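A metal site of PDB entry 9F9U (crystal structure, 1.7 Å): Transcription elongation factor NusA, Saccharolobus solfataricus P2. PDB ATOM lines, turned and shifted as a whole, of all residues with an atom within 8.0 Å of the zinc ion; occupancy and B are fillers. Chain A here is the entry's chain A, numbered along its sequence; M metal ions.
The side-chain sulfur (SG) of Cys 11 lies close to the backbone carbonyl oxygen (O) of Leu 16 (3.7 Å).
O of Cys 11 lies within hydrogen-bond range of OG of Ser 14, at 3.4 Å.
N of Arg 20 lies close to SG of Cys 18 (3.4 Å).
The side-chain carboxylate (OD1) of Asp 8 is in salt-bridge range of the guanidinium group (NH2) of Arg 20.
Within 4 Å of the zinc ion: Asp 8, Cys 11, Cys 18 and Cys 21.
Along chain A the residues within 4 Å of the zinc ion span positions 8 to 21.
The zinc ion is bound by the side-chain sulfur (SG) of Cys 11 (2.3 Å), the side-chain sulfur (SG) of Cys 18 (2.3 Å), the side-chain sulfur (SG) of Cys 21 (2.3 Å) and the side-chain carboxylate (OD2) of Asp 8 (2.3 Å).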
ATOM      1  N   PRO A   6      -3.614  -6.894  24.164  1.00  0.00           N
ATOM      2  CA  PRO A   6      -4.082  -7.892  25.145  1.00  0.00           C
ATOM      3  C   PRO A   6      -5.453  -8.501  24.818  1.00  0.00           C
ATOM      4  O   PRO A   6      -6.385  -7.817  24.398  1.00  0.00           O
ATOM      5  CB  PRO A   6      -4.111  -7.119  26.467  1.00  0.00           C
ATOM      6  CG  PRO A   6      -3.323  -5.843  26.209  1.00  0.00           C
ATOM      7  CD  PRO A   6      -3.490  -5.551  24.761  1.00  0.00           C
ATOM      8  N   LEU A   7      -5.548  -9.812  25.033  1.00  0.00           N
ATOM      9  CA  LEU A   7      -6.831 -10.514  25.067  1.00  0.00           C
ATOM     10  C   LEU A   7      -7.049 -11.033  26.482  1.00  0.00           C
ATOM     11  O   LEU A   7      -6.082 -11.322  27.190  1.00  0.00           O
ATOM     12  CB  LEU A   7      -6.868 -11.677  24.068  1.00  0.00           C
ATOM     13  CG  LEU A   7      -6.993 -11.386  22.571  1.00  0.00           C
ATOM     14  CD1 LEU A   7      -5.782 -10.681  21.992  1.00  0.00           C
ATOM     15  CD2 LEU A   7      -7.276 -12.668  21.800  1.00  0.00           C
ATOM     16  N   ASP A   8      -8.306 -11.212  26.879  1.00  0.00           N
ATOM     17  CA  ASP A   8      -8.590 -11.769  28.197  1.00  0.00           C
ATOM     18  C   ASP A   8      -8.151 -13.230  28.274  1.00  0.00           C
ATOM     19  O   ASP A   8      -8.353 -14.008  27.332  1.00  0.00           O
ATOM     20  CB  ASP A   8     -10.087 -11.681  28.507  1.00  0.00           C
ATOM     21  CG  ASP A   8     -10.593 -10.265  28.548  1.00  0.00           C
ATOM     22  OD1 ASP A   8     -10.200  -9.492  29.450  1.00  0.00           O
ATOM     23  OD2 ASP A   8     -11.369  -9.917  27.663  1.00  0.00           O
ATOM     24  N   TYR A   9      -7.580 -13.610  29.412  1.00  0.00           N
ATOM     25  CA  TYR A   9      -7.258 -15.014  29.646  1.00  0.00           C
ATOM     26  C   TYR A   9      -8.493 -15.895  29.463  1.00  0.00           C
ATOM     27  O   TYR A   9      -8.419 -16.963  28.849  1.00  0.00           O
ATOM     28  CB  TYR A   9      -6.696 -15.195  31.059  1.00  0.00           C
ATOM     29  CG  TYR A   9      -5.227 -14.988  31.238  1.00  0.00           C
ATOM     30  CD1 TYR A   9      -4.564 -13.978  30.550  1.00  0.00           C
ATOM     31  CD2 TYR A   9      -4.503 -15.760  32.137  1.00  0.00           C
ATOM     32  CE1 TYR A   9      -3.216 -13.754  30.741  1.00  0.00           C
ATOM     33  CE2 TYR A   9      -3.146 -15.555  32.333  1.00  0.00           C
ATOM     34  CZ  TYR A   9      -2.502 -14.547  31.634  1.00  0.00           C
ATOM     35  OH  TYR A   9      -1.155 -14.352  31.831  1.00  0.00           O
ATOM     36  N   VAL A  10      -9.661 -15.460  29.982  1.00  0.00           N
ATOM     37  CA  VAL A  10     -10.881 -16.268  29.907  1.00  0.00           C
ATOM     38  C   VAL A  10     -11.272 -16.529  28.461  1.00  0.00           C
ATOM     39  O   VAL A  10     -11.672 -17.643  28.089  1.00  0.00           O
ATOM     40  CB  VAL A  10     -12.025 -15.589  30.674  1.00  0.00           C
ATOM     41  CG1 VAL A  10     -13.378 -16.238  30.356  1.00  0.00           C
ATOM     42  CG2 VAL A  10     -11.744 -15.630  32.168  1.00  0.00           C
ATOM     43  N   CYS A  11     -11.242 -15.473  27.641  1.00  0.00           N
ATOM     44  CA  CYS A  11     -11.602 -15.605  26.230  1.00  0.00           C
ATOM     45  C   CYS A  11     -10.634 -16.509  25.481  1.00  0.00           C
ATOM     46  O   CYS A  11     -11.054 -17.336  24.661  1.00  0.00           O
ATOM     47  CB  CYS A  11     -11.642 -14.224  25.586  1.00  0.00           C
ATOM     48  SG  CYS A  11     -12.867 -13.166  26.342  1.00  0.00           S
ATOM     49  N   VAL A  12      -9.339 -16.319  25.697  1.00  0.00           N
ATOM     50  CA  VAL A  12      -8.342 -17.129  25.012  1.00  0.00           C
ATOM     51  C   VAL A  12      -8.500 -18.600  25.380  1.00  0.00           C
ATOM     52  O   VAL A  12      -8.497 -19.493  24.512  1.00  0.00           O
ATOM     53  CB  VAL A  12      -6.933 -16.613  25.340  1.00  0.00           C
ATOM     54  CG1 VAL A  12      -5.890 -17.592  24.835  1.00  0.00           C
ATOM     55  CG2 VAL A  12      -6.725 -15.211  24.743  1.00  0.00           C
ATOM     56  N   SER A  14     -11.000 -20.277  26.569  1.00  0.00           N
ATOM     57  CA  SER A  14     -12.277 -20.871  26.182  1.00  0.00           C
ATOM     58  C   SER A  14     -12.498 -20.853  24.686  1.00  0.00           C
ATOM     59  O   SER A  14     -13.214 -21.712  24.155  1.00  0.00           O
ATOM     60  CB  SER A  14     -13.436 -20.135  26.875  1.00  0.00           C
ATOM     61  OG  SER A  14     -13.547 -18.785  26.417  1.00  0.00           O
ATOM     62  N   LEU A  16     -14.198 -18.603  23.446  1.00  0.00           N
ATOM     63  CA  LEU A  16     -15.406 -17.793  23.395  1.00  0.00           C
ATOM     64  C   LEU A  16     -14.949 -16.358  23.601  1.00  0.00           C
ATOM     65  O   LEU A  16     -14.717 -15.929  24.740  1.00  0.00           O
ATOM     66  CB  LEU A  16     -16.396 -18.243  24.464  1.00  0.00           C
ATOM     67  CG  LEU A  16     -17.723 -17.491  24.553  1.00  0.00           C
ATOM     68  CD1 LEU A  16     -18.555 -17.738  23.297  1.00  0.00           C
ATOM     69  CD2 LEU A  16     -18.471 -17.913  25.800  1.00  0.00           C
ATOM     70  N   LEU A  17     -14.793 -15.626  22.517  1.00  0.00           N
ATOM     71  CA  LEU A  17     -14.279 -14.256  22.565  1.00  0.00           C
ATOM     72  C   LEU A  17     -15.398 -13.293  22.977  1.00  0.00           C
ATOM     73  O   LEU A  17     -16.444 -13.233  22.333  1.00  0.00           O
ATOM     74  CB  LEU A  17     -13.697 -13.860  21.212  1.00  0.00           C
ATOM     75  CG  LEU A  17     -12.678 -14.819  20.600  1.00  0.00           C
ATOM     76  CD1 LEU A  17     -12.115 -14.232  19.329  1.00  0.00           C
ATOM     77  CD2 LEU A  17     -11.556 -15.150  21.580  1.00  0.00           C
ATOM     78  N   CYS A  18     -15.154 -12.550  24.052  1.00  0.00           N
ATOM     79  CA  CYS A  18     -15.979 -11.422  24.475  1.00  0.00           C
ATOM     80  C   CYS A  18     -16.055 -10.340  23.410  1.00  0.00           C
ATOM     81  O   CYS A  18     -15.382 -10.412  22.383  1.00  0.00           O
ATOM     82  CB  CYS A  18     -15.432 -10.855  25.795  1.00  0.00           C
ATOM     83  SG  CYS A  18     -14.109  -9.633  25.615  1.00  0.00           S
ATOM     84  N   ASN A  19     -16.861  -9.294  23.636  1.00  0.00           N
ATOM     85  CA  ASN A  19     -17.051  -8.282  22.611  1.00  0.00           C
ATOM     86  C   ASN A  19     -15.732  -7.600  22.236  1.00  0.00           C
ATOM     87  O   ASN A  19     -15.463  -7.364  21.045  1.00  0.00           O
ATOM     88  CB  ASN A  19     -18.062  -7.246  23.096  1.00  0.00           C
ATOM     89  CG  ASN A  19     -18.381  -6.225  22.042  1.00  0.00           C
ATOM     90  OD1 ASN A  19     -17.663  -5.228  21.849  1.00  0.00           O
ATOM     91  ND2 ASN A  19     -19.471  -6.467  21.314  1.00  0.00           N
ATOM     92  N   ARG A  20     -14.905  -7.303  23.236  1.00  0.00           N
ATOM     93  CA  ARG A  20     -13.624  -6.653  22.998  1.00  0.00           C
ATOM     94  C   ARG A  20     -12.702  -7.538  22.182  1.00  0.00           C
ATOM     95  O   ARG A  20     -12.117  -7.101  21.179  1.00  0.00           O
ATOM     96  CB  ARG A  20     -12.975  -6.340  24.344  1.00  0.00           C
ATOM     97  CG  ARG A  20     -13.714  -5.302  25.189  1.00  0.00           C
ATOM     98  CD  ARG A  20     -12.950  -4.936  26.468  1.00  0.00           C
ATOM     99  NE  ARG A  20     -12.185  -6.064  26.982  1.00  0.00           N
ATOM    100  CZ  ARG A  20     -10.862  -6.189  26.907  1.00  0.00           C
ATOM    101  NH1 ARG A  20     -10.102  -5.193  26.471  1.00  0.00           N
ATOM    102  NH2 ARG A  20     -10.299  -7.342  27.263  1.00  0.00           N
ATOM    103  N   CYS A  21     -12.557  -8.806  22.604  1.00  0.00           N
ATOM    104  CA  CYS A  21     -11.602  -9.676  21.919  1.00  0.00           C
ATOM    105  C   CYS A  21     -12.087  -9.987  20.509  1.00  0.00           C
ATOM    106  O   CYS A  21     -11.288 -10.058  19.559  1.00  0.00           O
ATOM    107  CB  CYS A  21     -11.378 -10.933  22.751  1.00  0.00           C
ATOM    108  SG  CYS A  21     -10.550 -10.533  24.353  1.00  0.00           S
ATOM    109  N   GLN A  22     -13.404 -10.138  20.335  1.00  0.00           N
ATOM    110  CA  GLN A  22     -13.951 -10.381  19.000  1.00  0.00           C
ATOM    111  C   GLN A  22     -13.712  -9.187  18.090  1.00  0.00           C
ATOM    112  O   GLN A  22     -13.473  -9.340  16.886  1.00  0.00           O
ATOM    113  CB  GLN A  22     -15.445 -10.667  19.080  1.00  0.00           C
ATOM    114  CG  GLN A  22     -16.075 -10.998  17.749  1.00  0.00           C
ATOM    115  CD  GLN A  22     -15.435 -12.238  17.146  1.00  0.00           C
ATOM    116  OE1 GLN A  22     -14.729 -12.185  16.136  1.00  0.00           O
ATOM    117  NE2 GLN A  22     -15.629 -13.360  17.818  1.00  0.00           N
ATOM    118  N   SER A  23     -13.790  -7.978  18.644  1.00  0.00           N
ATOM    119  CA  SER A  23     -13.537  -6.780  17.856  1.00  0.00           C
ATOM    120  C   SER A  23     -12.098  -6.763  17.348  1.00  0.00           C
ATOM    121  O   SER A  23     -11.837  -6.352  16.212  1.00  0.00           O
ATOM    122  CB  SER A  23     -13.889  -5.537  18.677  1.00  0.00           C
ATOM    123  OG  SER A  23     -12.811  -5.159  19.518  1.00  0.00           O
ATOM    124  N   LEU A  24     -11.141  -7.255  18.159  1.00  0.00           N
ATOM    125  CA  LEU A  24      -9.766  -7.299  17.692  1.00  0.00           C
ATOM    126  C   LEU A  24      -9.618  -8.250  16.515  1.00  0.00           C
ATOM    127  O   LEU A  24      -8.813  -8.005  15.613  1.00  0.00           O
ATOM    128  CB  LEU A  24      -8.793  -7.698  18.811  1.00  0.00           C
ATOM    129  CG  LEU A  24      -8.682  -6.769  20.025  1.00  0.00           C
ATOM    130  CD1 LEU A  24      -7.908  -7.445  21.152  1.00  0.00           C
ATOM    131  CD2 LEU A  24      -8.077  -5.406  19.660  1.00  0.00           C
HETATM  132 ZN    ZN M   1     -12.272 -11.009  25.812  1.00  0.00          ZN
